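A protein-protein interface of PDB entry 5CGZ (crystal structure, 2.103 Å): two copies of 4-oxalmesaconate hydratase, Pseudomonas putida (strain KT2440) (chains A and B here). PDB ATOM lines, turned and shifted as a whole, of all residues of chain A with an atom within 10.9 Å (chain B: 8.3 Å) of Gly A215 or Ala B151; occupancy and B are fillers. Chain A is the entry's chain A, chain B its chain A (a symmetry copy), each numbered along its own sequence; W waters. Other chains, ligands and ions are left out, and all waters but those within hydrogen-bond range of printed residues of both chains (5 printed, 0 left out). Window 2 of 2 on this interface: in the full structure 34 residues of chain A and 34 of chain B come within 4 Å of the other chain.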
ATOM      1  N   PHE A 172     -19.368  16.994  35.592  1.00  0.00           N
ATOM      2  CA  PHE A 172     -19.641  18.176  36.411  1.00  0.00           C
ATOM      3  C   PHE A 172     -20.789  18.976  35.826  1.00  0.00           C
ATOM      4  O   PHE A 172     -20.771  19.353  34.646  1.00  0.00           O
ATOM      5  CB  PHE A 172     -18.410  19.087  36.538  1.00  0.00           C
ATOM      6  CG  PHE A 172     -17.336  18.536  37.427  1.00  0.00           C
ATOM      7  CD1 PHE A 172     -17.558  18.385  38.787  1.00  0.00           C
ATOM      8  CD2 PHE A 172     -16.098  18.187  36.906  1.00  0.00           C
ATOM      9  CE1 PHE A 172     -16.564  17.874  39.620  1.00  0.00           C
ATOM     10  CE2 PHE A 172     -15.097  17.685  37.727  1.00  0.00           C
ATOM     11  CZ  PHE A 172     -15.334  17.522  39.088  1.00  0.00           C
ATOM     12  N   GLY A 207     -16.660  23.535  41.677  1.00  0.00           N
ATOM     13  CA  GLY A 207     -16.666  24.643  40.735  1.00  0.00           C
ATOM     14  C   GLY A 207     -15.279  24.904  40.170  1.00  0.00           C
ATOM     15  O   GLY A 207     -15.105  25.044  38.957  1.00  0.00           O
ATOM     16  N   VAL A 208     -14.286  24.971  41.050  1.00  0.00           N
ATOM     17  CA  VAL A 208     -12.908  25.191  40.612  1.00  0.00           C
ATOM     18  C   VAL A 208     -12.432  24.037  39.734  1.00  0.00           C
ATOM     19  O   VAL A 208     -11.791  24.257  38.707  1.00  0.00           O
ATOM     20  CB  VAL A 208     -11.944  25.366  41.816  1.00  0.00           C
ATOM     21  CG1 VAL A 208     -10.480  25.293  41.363  1.00  0.00           C
ATOM     22  CG2 VAL A 208     -12.216  26.695  42.529  1.00  0.00           C
ATOM     23  N   GLN A 209     -12.760  22.805  40.125  1.00  0.00           N
ATOM     24  CA  GLN A 209     -12.329  21.634  39.361  1.00  0.00           C
ATOM     25  C   GLN A 209     -13.002  21.572  37.989  1.00  0.00           C
ATOM     26  O   GLN A 209     -12.361  21.237  37.001  1.00  0.00           O
ATOM     27  CB  GLN A 209     -12.601  20.347  40.142  1.00  0.00           C
ATOM     28  CG  GLN A 209     -11.844  20.274  41.475  1.00  0.00           C
ATOM     29  CD  GLN A 209     -12.329  19.132  42.361  1.00  0.00           C
ATOM     30  OE1 GLN A 209     -13.101  18.277  41.925  1.00  0.00           O
ATOM     31  NE2 GLN A 209     -11.878  19.118  43.611  1.00  0.00           N
ATOM     32  N   ALA A 210     -14.294  21.887  37.934  1.00  0.00           N
ATOM     33  CA  ALA A 210     -15.002  21.943  36.661  1.00  0.00           C
ATOM     34  C   ALA A 210     -14.365  22.995  35.747  1.00  0.00           C
ATOM     35  O   ALA A 210     -14.128  22.745  34.561  1.00  0.00           O
ATOM     36  CB  ALA A 210     -16.488  22.246  36.884  1.00  0.00           C
ATOM     37  N   LYS A 211     -14.072  24.165  36.311  1.00  0.00           N
ATOM     38  CA  LYS A 211     -13.415  25.224  35.549  1.00  0.00           C
ATOM     39  C   LYS A 211     -12.080  24.730  34.998  1.00  0.00           C
ATOM     40  O   LYS A 211     -11.753  24.957  33.829  1.00  0.00           O
ATOM     41  CB  LYS A 211     -13.213  26.477  36.411  1.00  0.00           C
ATOM     42  CG  LYS A 211     -12.538  27.625  35.657  1.00  0.00           C
ATOM     43  CD  LYS A 211     -13.349  27.973  34.396  1.00  0.00           C
ATOM     44  CE  LYS A 211     -12.709  29.093  33.587  1.00  0.00           C
ATOM     45  NZ  LYS A 211     -12.623  30.357  34.365  1.00  0.00           N
ATOM     46  N   ARG A 212     -11.319  24.024  35.829  1.00  0.00           N
ATOM     47  CA  ARG A 212     -10.032  23.491  35.382  1.00  0.00           C
ATOM     48  C   ARG A 212     -10.243  22.570  34.180  1.00  0.00           C
ATOM     49  O   ARG A 212      -9.427  22.528  33.264  1.00  0.00           O
ATOM     50  CB  ARG A 212      -9.326  22.744  36.521  1.00  0.00           C
ATOM     51  CG  ARG A 212      -7.927  22.198  36.177  1.00  0.00           C
ATOM     52  CD  ARG A 212      -6.938  23.324  35.856  1.00  0.00           C
ATOM     53  NE  ARG A 212      -5.579  23.053  36.338  1.00  0.00           N
ATOM     54  CZ  ARG A 212      -4.655  22.364  35.664  1.00  0.00           C
ATOM     55  NH1 ARG A 212      -4.923  21.862  34.459  1.00  0.00           N
ATOM     56  NH2 ARG A 212      -3.452  22.171  36.199  1.00  0.00           N
ATOM     57  N   ASN A 213     -11.358  21.850  34.164  1.00  0.00           N
ATOM     58  CA  ASN A 213     -11.571  20.878  33.102  1.00  0.00           C
ATOM     59  C   ASN A 213     -12.217  21.470  31.846  1.00  0.00           C
ATOM     60  O   ASN A 213     -12.515  20.728  30.917  1.00  0.00           O
ATOM     61  CB  ASN A 213     -12.403  19.706  33.620  1.00  0.00           C
ATOM     62  CG  ASN A 213     -11.576  18.739  34.452  1.00  0.00           C
ATOM     63  OD1 ASN A 213     -10.878  17.873  33.909  1.00  0.00           O
ATOM     64  ND2 ASN A 213     -11.637  18.890  35.773  1.00  0.00           N
ATOM     65  N   VAL A 214     -12.421  22.791  31.814  1.00  0.00           N
ATOM     66  CA  VAL A 214     -12.779  23.461  30.558  1.00  0.00           C
ATOM     67  C   VAL A 214     -11.676  24.417  30.111  1.00  0.00           C
ATOM     68  O   VAL A 214     -11.806  25.084  29.094  1.00  0.00           O
ATOM     69  CB  VAL A 214     -14.107  24.254  30.653  1.00  0.00           C
ATOM     70  CG1 VAL A 214     -15.253  23.338  31.056  1.00  0.00           C
ATOM     71  CG2 VAL A 214     -13.976  25.437  31.624  1.00  0.00           C
ATOM     72  N   GLY A 215     -10.587  24.474  30.872  1.00  0.00           N
ATOM     73  CA  GLY A 215      -9.488  25.371  30.551  1.00  0.00           C
ATOM     74  C   GLY A 215      -9.415  26.500  31.557  1.00  0.00           C
ATOM     75  O   GLY A 215     -10.352  27.290  31.681  1.00  0.00           O
ATOM     76  N   ILE A 216      -8.303  26.582  32.282  1.00  0.00           N
ATOM     77  CA  ILE A 216      -8.218  27.500  33.408  1.00  0.00           C
ATOM     78  C   ILE A 216      -8.300  28.973  32.972  1.00  0.00           C
ATOM     79  O   ILE A 216      -8.681  29.831  33.764  1.00  0.00           O
ATOM     80  CB  ILE A 216      -6.920  27.259  34.229  1.00  0.00           C
ATOM     81  CG1 ILE A 216      -7.078  27.816  35.651  1.00  0.00           C
ATOM     82  CG2 ILE A 216      -5.699  27.843  33.517  1.00  0.00           C
ATOM     83  CD1 ILE A 216      -6.010  27.350  36.629  1.00  0.00           C
ATOM     84  N   THR A 217      -7.985  29.267  31.712  1.00  0.00           N
ATOM     85  CA  THR A 217      -8.090  30.645  31.235  1.00  0.00           C
ATOM     86  C   THR A 217      -9.361  30.899  30.420  1.00  0.00           C
ATOM     87  O   THR A 217      -9.527  31.977  29.863  1.00  0.00           O
ATOM     88  CB  THR A 217      -6.873  31.053  30.372  1.00  0.00           C
ATOM     89  OG1 THR A 217      -6.823  30.244  29.190  1.00  0.00           O
ATOM     90  CG2 THR A 217      -5.573  30.896  31.162  1.00  0.00           C
ATOM     91  N   SER A 218     -10.245  29.911  30.340  1.00  0.00           N
ATOM     92  CA  SER A 218     -11.538  30.091  29.677  1.00  0.00           C
ATOM     93  C   SER A 218     -12.321  31.238  30.311  1.00  0.00           C
ATOM     94  O   SER A 218     -12.176  31.504  31.503  1.00  0.00           O
ATOM     95  CB  SER A 218     -12.364  28.798  29.745  1.00  0.00           C
ATOM     96  OG  SER A 218     -13.748  29.058  29.541  1.00  0.00           O
ATOM     97  N   ALA A 219     -13.156  31.911  29.521  1.00  0.00           N
ATOM     98  CA  ALA A 219     -13.975  33.004  30.050  1.00  0.00           C
ATOM     99  C   ALA A 219     -15.234  32.504  30.746  1.00  0.00           C
ATOM    100  O   ALA A 219     -15.976  33.305  31.310  1.00  0.00           O
ATOM    101  CB  ALA A 219     -14.363  33.989  28.927  1.00  0.00           C
ATOM    102  N   ARG A 220     -15.495  31.197  30.692  1.00  0.00           N
ATOM    103  CA  ARG A 220     -16.680  30.645  31.344  1.00  0.00           C
ATOM    104  C   ARG A 220     -16.602  30.892  32.847  1.00  0.00           C
ATOM    105  O   ARG A 220     -15.541  30.758  33.462  1.00  0.00           O
ATOM    106  CB  ARG A 220     -16.833  29.149  31.042  1.00  0.00           C
ATOM    107  CG  ARG A 220     -17.109  28.871  29.574  1.00  0.00           C
ATOM    108  CD  ARG A 220     -17.138  27.385  29.255  1.00  0.00           C
ATOM    109  NE  ARG A 220     -18.265  26.708  29.897  1.00  0.00           N
ATOM    110  CZ  ARG A 220     -18.542  25.412  29.751  1.00  0.00           C
ATOM    111  NH1 ARG A 220     -17.776  24.642  28.983  1.00  0.00           N
ATOM    112  NH2 ARG A 220     -19.583  24.884  30.370  1.00  0.00           N
ATOM    113  N   ASN A 221     -17.734  31.277  33.423  1.00  0.00           N
ATOM    114  CA  ASN A 221     -17.797  31.720  34.808  1.00  0.00           C
ATOM    115  C   ASN A 221     -18.325  30.598  35.696  1.00  0.00           C
ATOM    116  O   ASN A 221     -19.462  30.642  36.154  1.00  0.00           O
ATOM    117  CB  ASN A 221     -18.684  32.966  34.912  1.00  0.00           C
ATOM    118  CG  ASN A 221     -18.789  33.491  36.331  1.00  0.00           C
ATOM    119  OD1 ASN A 221     -17.803  33.527  37.063  1.00  0.00           O
ATOM    120  ND2 ASN A 221     -19.994  33.890  36.728  1.00  0.00           N
ATOM    121  N   ILE A 222     -17.514  29.568  35.909  1.00  0.00           N
ATOM    122  CA  ILE A 222     -17.998  28.388  36.618  1.00  0.00           C
ATOM    123  C   ILE A 222     -17.578  28.474  38.078  1.00  0.00           C
ATOM    124  O   ILE A 222     -16.409  28.273  38.409  1.00  0.00           O
ATOM    125  CB  ILE A 222     -17.476  27.092  35.974  1.00  0.00           C
ATOM    126  CG1 ILE A 222     -17.835  27.074  34.480  1.00  0.00           C
ATOM    127  CG2 ILE A 222     -18.068  25.886  36.680  1.00  0.00           C
ATOM    128  CD1 ILE A 222     -17.238  25.899  33.698  1.00  0.00           C
ATOM    129  N   LEU A 239     -17.880  14.895  20.191  1.00  0.00           N
ATOM    130  CA  LEU A 239     -16.944  14.560  21.269  1.00  0.00           C
ATOM    131  C   LEU A 239     -16.335  15.762  21.984  1.00  0.00           C
ATOM    132  O   LEU A 239     -15.491  15.585  22.858  1.00  0.00           O
ATOM    133  CB  LEU A 239     -15.811  13.676  20.726  1.00  0.00           C
ATOM    134  CG  LEU A 239     -16.270  12.283  20.281  1.00  0.00           C
ATOM    135  CD1 LEU A 239     -15.118  11.482  19.703  1.00  0.00           C
ATOM    136  CD2 LEU A 239     -16.949  11.518  21.428  1.00  0.00           C
ATOM    137  N   ALA A 240     -16.755  16.976  21.634  1.00  0.00           N
ATOM    138  CA  ALA A 240     -16.193  18.170  22.274  1.00  0.00           C
ATOM    139  C   ALA A 240     -16.656  18.287  23.729  1.00  0.00           C
ATOM    140  O   ALA A 240     -16.063  19.015  24.537  1.00  0.00           O
ATOM    141  CB  ALA A 240     -16.569  19.426  21.501  1.00  0.00           C
ATOM    142  OXT ALA A 240     -17.643  17.650  24.118  1.00  0.00           O
ATOM    143  N   TYR B 102      -0.209  20.627  18.844  1.00  0.00           N
ATOM    144  CA  TYR B 102      -1.310  21.109  19.680  1.00  0.00           C
ATOM    145  C   TYR B 102      -1.467  22.620  19.576  1.00  0.00           C
ATOM    146  O   TYR B 102      -2.581  23.129  19.431  1.00  0.00           O
ATOM    147  CB  TYR B 102      -1.089  20.741  21.150  1.00  0.00           C
ATOM    148  CG  TYR B 102      -1.646  19.400  21.603  1.00  0.00           C
ATOM    149  CD1 TYR B 102      -2.956  19.287  22.064  1.00  0.00           C
ATOM    150  CD2 TYR B 102      -0.842  18.259  21.626  1.00  0.00           C
ATOM    151  CE1 TYR B 102      -3.465  18.060  22.511  1.00  0.00           C
ATOM    152  CE2 TYR B 102      -1.340  17.026  22.077  1.00  0.00           C
ATOM    153  CZ  TYR B 102      -2.651  16.938  22.514  1.00  0.00           C
ATOM    154  OH  TYR B 102      -3.145  15.730  22.955  1.00  0.00           O
ATOM    155  N   GLN B 106      -4.846  23.609  17.912  1.00  0.00           N
ATOM    156  CA  GLN B 106      -5.783  24.005  18.968  1.00  0.00           C
ATOM    157  C   GLN B 106      -7.023  23.098  19.002  1.00  0.00           C
ATOM    158  O   GLN B 106      -8.156  23.572  18.920  1.00  0.00           O
ATOM    159  CB  GLN B 106      -6.199  25.468  18.776  1.00  0.00           C
ATOM    160  CG  GLN B 106      -5.047  26.473  18.925  1.00  0.00           C
ATOM    161  CD  GLN B 106      -4.702  26.750  20.380  1.00  0.00           C
ATOM    162  OE1 GLN B 106      -5.538  26.587  21.268  1.00  0.00           O
ATOM    163  NE2 GLN B 106      -3.463  27.164  20.631  1.00  0.00           N
ATOM    164  N   PRO B 107      -6.815  21.781  19.123  1.00  0.00           N
ATOM    165  CA  PRO B 107      -7.942  20.845  18.979  1.00  0.00           C
ATOM    166  C   PRO B 107      -8.997  20.974  20.082  1.00  0.00           C
ATOM    167  O   PRO B 107      -8.666  21.311  21.224  1.00  0.00           O
ATOM    168  CB  PRO B 107      -7.263  19.473  19.036  1.00  0.00           C
ATOM    169  CG  PRO B 107      -6.020  19.708  19.872  1.00  0.00           C
ATOM    170  CD  PRO B 107      -5.557  21.102  19.498  1.00  0.00           C
ATOM    171  N   GLU B 108     -10.256  20.706  19.734  1.00  0.00           N
ATOM    172  CA  GLU B 108     -11.344  20.696  20.709  1.00  0.00           C
ATOM    173  C   GLU B 108     -11.385  19.390  21.479  1.00  0.00           C
ATOM    174  O   GLU B 108     -11.934  19.329  22.581  1.00  0.00           O
ATOM    175  CB  GLU B 108     -12.696  20.910  20.034  1.00  0.00           C
ATOM    176  CG  GLU B 108     -12.962  22.346  19.607  1.00  0.00           C
ATOM    177  CD  GLU B 108     -14.364  22.513  19.040  1.00  0.00           C
ATOM    178  OE1 GLU B 108     -15.243  21.645  19.301  1.00  0.00           O
ATOM    179  OE2 GLU B 108     -14.586  23.511  18.329  1.00  0.00           O
ATOM    180  N   PHE B 109     -10.837  18.338  20.878  1.00  0.00           N
ATOM    181  CA  PHE B 109     -10.722  17.056  21.564  1.00  0.00           C
ATOM    182  C   PHE B 109      -9.614  16.242  20.918  1.00  0.00           C
ATOM    183  O   PHE B 109      -9.161  16.561  19.810  1.00  0.00           O
ATOM    184  CB  PHE B 109     -12.061  16.289  21.557  1.00  0.00           C
ATOM    185  CG  PHE B 109     -12.542  15.873  20.180  1.00  0.00           C
ATOM    186  CD1 PHE B 109     -12.132  14.669  19.619  1.00  0.00           C
ATOM    187  CD2 PHE B 109     -13.433  16.669  19.469  1.00  0.00           C
ATOM    188  CE1 PHE B 109     -12.583  14.274  18.360  1.00  0.00           C
ATOM    189  CE2 PHE B 109     -13.891  16.283  18.212  1.00  0.00           C
ATOM    190  CZ  PHE B 109     -13.464  15.085  17.654  1.00  0.00           C
ATOM    191  N   VAL B 110      -9.163  15.211  21.628  1.00  0.00           N
ATOM    192  CA  VAL B 110      -8.073  14.362  21.161  1.00  0.00           C
ATOM    193  C   VAL B 110      -8.458  12.885  21.246  1.00  0.00           C
ATOM    194  O   VAL B 110      -9.033  12.442  22.241  1.00  0.00           O
ATOM    195  CB  VAL B 110      -6.796  14.593  21.986  1.00  0.00           C
ATOM    196  CG1 VAL B 110      -5.616  13.847  21.363  1.00  0.00           C
ATOM    197  CG2 VAL B 110      -6.505  16.079  22.095  1.00  0.00           C
ATOM    198  N   ARG B 134      -0.123  17.586  25.390  1.00  0.00           N
ATOM    199  CA  ARG B 134      -1.271  18.441  25.659  1.00  0.00           C
ATOM    200  C   ARG B 134      -1.021  19.359  26.857  1.00  0.00           C
ATOM    201  O   ARG B 134      -1.324  20.560  26.818  1.00  0.00           O
ATOM    202  CB  ARG B 134      -2.509  17.571  25.902  1.00  0.00           C
ATOM    203  CG  ARG B 134      -3.792  18.304  26.260  1.00  0.00           C
ATOM    204  CD  ARG B 134      -4.899  17.249  26.396  1.00  0.00           C
ATOM    205  NE  ARG B 134      -6.120  17.738  27.033  1.00  0.00           N
ATOM    206  CZ  ARG B 134      -6.267  17.938  28.343  1.00  0.00           C
ATOM    207  NH1 ARG B 134      -5.257  17.721  29.184  1.00  0.00           N
ATOM    208  NH2 ARG B 134      -7.431  18.370  28.808  1.00  0.00           N
ATOM    209  N   GLN B 138      -0.338  23.554  27.346  1.00  0.00           N
ATOM    210  CA  GLN B 138      -1.094  24.404  28.264  1.00  0.00           C
ATOM    211  C   GLN B 138      -0.217  25.424  29.006  1.00  0.00           C
ATOM    212  O   GLN B 138      -0.724  26.397  29.561  1.00  0.00           O
ATOM    213  CB  GLN B 138      -1.822  23.549  29.306  1.00  0.00           C
ATOM    214  CG  GLN B 138      -2.940  22.655  28.776  1.00  0.00           C
ATOM    215  CD  GLN B 138      -3.510  21.772  29.883  1.00  0.00           C
ATOM    216  OE1 GLN B 138      -2.787  21.396  30.811  1.00  0.00           O
ATOM    217  NE2 GLN B 138      -4.805  21.441  29.795  1.00  0.00           N
ATOM    218  N   ILE B 148      -1.853  29.553  24.299  1.00  0.00           N
ATOM    219  CA  ILE B 148      -1.821  28.251  24.956  1.00  0.00           C
ATOM    220  C   ILE B 148      -3.038  27.414  24.582  1.00  0.00           C
ATOM    221  O   ILE B 148      -4.041  27.926  24.081  1.00  0.00           O
ATOM    222  CB  ILE B 148      -1.759  28.375  26.498  1.00  0.00           C
ATOM    223  CG1 ILE B 148      -3.072  28.937  27.049  1.00  0.00           C
ATOM    224  CG2 ILE B 148      -0.573  29.234  26.923  1.00  0.00           C
ATOM    225  CD1 ILE B 148      -3.094  29.068  28.555  1.00  0.00           C
ATOM    226  N   VAL B 149      -2.930  26.117  24.826  1.00  0.00           N
ATOM    227  CA  VAL B 149      -4.040  25.188  24.667  1.00  0.00           C
ATOM    228  C   VAL B 149      -4.927  25.231  25.919  1.00  0.00           C
ATOM    229  O   VAL B 149      -4.435  25.498  27.024  1.00  0.00           O
ATOM    230  CB  VAL B 149      -3.503  23.764  24.409  1.00  0.00           C
ATOM    231  CG1 VAL B 149      -4.487  22.705  24.851  1.00  0.00           C
ATOM    232  CG2 VAL B 149      -3.124  23.610  22.936  1.00  0.00           C
ATOM    233  N   GLY B 150      -6.226  24.993  25.748  1.00  0.00           N
ATOM    234  CA  GLY B 150      -7.147  24.930  26.879  1.00  0.00           C
ATOM    235  C   GLY B 150      -7.169  23.534  27.496  1.00  0.00           C
ATOM    236  O   GLY B 150      -6.119  22.990  27.843  1.00  0.00           O
ATOM    237  N   ALA B 151      -8.358  22.946  27.617  1.00  0.00           N
ATOM    238  CA  ALA B 151      -8.492  21.605  28.187  1.00  0.00           C
ATOM    239  C   ALA B 151      -9.359  20.717  27.306  1.00  0.00           C
ATOM    240  O   ALA B 151     -10.435  20.301  27.720  1.00  0.00           O
ATOM    241  CB  ALA B 151      -9.074  21.678  29.607  1.00  0.00           C
ATOM    242  N   PRO B 152      -8.900  20.432  26.078  1.00  0.00           N
ATOM    243  CA  PRO B 152      -9.704  19.563  25.210  1.00  0.00           C
ATOM    244  C   PRO B 152      -9.835  18.175  25.820  1.00  0.00           C
ATOM    245  O   PRO B 152      -8.842  17.637  26.306  1.00  0.00           O
ATOM    246  CB  PRO B 152      -8.902  19.517  23.898  1.00  0.00           C
ATOM    247  CG  PRO B 152      -7.477  19.837  24.318  1.00  0.00           C
ATOM    248  CD  PRO B 152      -7.614  20.814  25.462  1.00  0.00           C
ATOM    249  N   PRO B 153     -11.050  17.622  25.827  1.00  0.00           N
ATOM    250  CA  PRO B 153     -11.244  16.231  26.252  1.00  0.00           C
ATOM    251  C   PRO B 153     -10.316  15.284  25.492  1.00  0.00           C
ATOM    252  O   PRO B 153     -10.013  15.501  24.318  1.00  0.00           O
ATOM    253  CB  PRO B 153     -12.716  15.957  25.910  1.00  0.00           C
ATOM    254  CG  PRO B 153     -13.376  17.317  25.995  1.00  0.00           C
ATOM    255  CD  PRO B 153     -12.321  18.301  25.503  1.00  0.00           C
ATOM    256  N   VAL B 154      -9.841  14.254  26.179  1.00  0.00           N
ATOM    257  CA  VAL B 154      -9.020  13.226  25.561  1.00  0.00           C
ATOM    258  C   VAL B 154      -9.760  11.888  25.689  1.00  0.00           C
ATOM    259  O   VAL B 154     -10.325  11.589  26.739  1.00  0.00           O
ATOM    260  CB  VAL B 154      -7.633  13.135  26.224  1.00  0.00           C
ATOM    261  CG1 VAL B 154      -6.801  12.013  25.589  1.00  0.00           C
ATOM    262  CG2 VAL B 154      -6.899  14.478  26.137  1.00  0.00           C
ATOM    263  N   PHE B 232     -10.915  12.606  31.010  1.00  0.00           N
ATOM    264  CA  PHE B 232     -11.292  13.648  31.959  1.00  0.00           C
ATOM    265  C   PHE B 232     -12.799  13.720  32.172  1.00  0.00           C
ATOM    266  O   PHE B 232     -13.576  13.357  31.284  1.00  0.00           O
ATOM    267  CB  PHE B 232     -10.789  15.022  31.486  1.00  0.00           C
ATOM    268  CG  PHE B 232      -9.308  15.075  31.273  1.00  0.00           C
ATOM    269  CD1 PHE B 232      -8.446  15.162  32.357  1.00  0.00           C
ATOM    270  CD2 PHE B 232      -8.779  15.021  29.991  1.00  0.00           C
ATOM    271  CE1 PHE B 232      -7.073  15.196  32.172  1.00  0.00           C
ATOM    272  CE2 PHE B 232      -7.400  15.051  29.787  1.00  0.00           C
ATOM    273  CZ  PHE B 232      -6.546  15.133  30.874  1.00  0.00           C
ATOM    274  N   PRO B 233     -13.214  14.219  33.345  1.00  0.00           N
ATOM    275  CA  PRO B 233     -14.631  14.493  33.595  1.00  0.00           C
ATOM    276  C   PRO B 233     -15.154  15.544  32.619  1.00  0.00           C
ATOM    277  O   PRO B 233     -14.469  16.531  32.352  1.00  0.00           O
ATOM    278  CB  PRO B 233     -14.637  15.025  35.032  1.00  0.00           C
ATOM    279  CG  PRO B 233     -13.247  15.604  35.220  1.00  0.00           C
ATOM    280  CD  PRO B 233     -12.347  14.677  34.453  1.00  0.00           C
ATOM    281  N   VAL B 235     -17.872  18.572  31.453  1.00  0.00           N
ATOM    282  CA  VAL B 235     -18.582  19.660  32.111  1.00  0.00           C
ATOM    283  C   VAL B 235     -19.814  19.997  31.290  1.00  0.00           C
ATOM    284  O   VAL B 235     -19.716  20.196  30.081  1.00  0.00           O
ATOM    285  CB  VAL B 235     -17.705  20.914  32.251  1.00  0.00           C
ATOM    286  CG1 VAL B 235     -18.489  22.040  32.934  1.00  0.00           C
ATOM    287  CG2 VAL B 235     -16.431  20.590  33.021  1.00  0.00           C
HETATM  288  O   HOH W   1      -6.845  21.843  32.582  1.00  0.00           O
HETATM  289  O   HOH W   2      -9.516  18.466  31.547  1.00  0.00           O
HETATM  290  O   HOH W   3     -20.632  22.627  28.934  1.00  0.00           O
HETATM  291  O   HOH W   4     -14.067  20.799  23.836  1.00  0.00           O
HETATM  292  O   HOH W   5      -3.297  19.864  33.012  1.00  0.00           O
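The side-chain amide nitrogen (ND2) of Asn A213 is in hydrogen-bond range of the backbone carbonyl oxygen (O) of Gln A209, at 2.7 Å.
OE1 of Gln B106 sits close to O of Ile B148 (3.5 Å).
The backbone NH (N) of Arg A220 is in hydrogen-bond range of the side-chain hydroxyl (OG) of Ser A218 (3.0 Å).
The backbone carbonyl oxygen (O) of Pro B153 sits at hydrogen-bond distance from the backbone NH (N) of Val B110, at 2.8 Å.
NZ of Lys A211 lies within hydrogen-bond range of O of Arg A220.
Water W1 lies within hydrogen-bond range of the guanidinium group (NH1) of Arg A212 (2.7 Å) and the side-chain amide nitrogen (NE2) of Gln B138 (3.5 Å).
Water W5 lies within hydrogen-bond range of the side-chain amide oxygen (OE1) of Gln B138 (2.7 Å) and the guanidinium group (NH1) of Arg A212 (3.0 Å).
Water W4 lies within hydrogen-bond range of the chain-end carboxylate (O) of Ala A240 (2.8 Å) and the backbone carbonyl oxygen (O) of Glu B108 (2.9 Å).
Water W2 lies within hydrogen-bond range of OD1 of Asn A213 (2.8 Å) and NH2 of Arg B134 (3.4 Å).
Water W3 lies within hydrogen-bond range of O of Val B235 (2.8 Å) and NH2 of Arg A220 (2.9 Å).
Hydrophobic or aromatic side chains of chain B that line the printed part of chain A: Phe B109, Ile B148, Ala B151, Pro B153, Phe B232, Pro B233 and Val B235.
Printed residues of chain B within 4 Å of Phe A172: Pro B233 (3.7 Å) and Val B235 (3.4 Å).
Printed residues of chain B within 4 Å of Arg A212: Ala B151.
Gly A215 touches just one residue of chain B: Ala B151 (3.4 Å).
Val B149 touches none of the printed residues of chain A.
No residue of chain A comes within 4 Å of Gly B150.
Of chain A, only Arg A212 (3.8 Å), Asn A213 (3.8 Å), Val A214 (3.8 Å) and Gly A215 (3.4 Å) come within 4 Å of Ala B151.
Of chain A, only Ala A240 comes within 4 Å of Pro B153.
The nearest residue of chain B that does not touch Gly A215 is Gly B150 (4.3 Å).
No position is printed for both chains.
Among the printed residues, pairs that only touch across the chains: Phe A172 with Val B235 (3.4 Å), Ala A240 with Glu B108 (3.4 Å), Gly A215 with Ala B151 (3.4 Å), Ala A240 with Pro B153 (3.5 Å), Ala A210 with Val B235 (3.5 Å), Asn A213 with Pro B233 (3.5 Å), Val A214 with Val B235 (3.6 Å), Leu A239 with Phe B109 (3.7 Å), Asn A213 with Phe B232 (3.7 Å), Phe A172 with Pro B233 (3.7 Å), Arg A212 with Ala B151 (3.8 Å), Asn A213 with Ala B151 (3.8 Å), Val A214 with Ala B151 (3.8 Å), Thr A217 with Ile B148 (3.96 Å), Ala A240 with Phe B109 (3.98 Å) and Arg A220 with Val B235 (3.98 Å).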
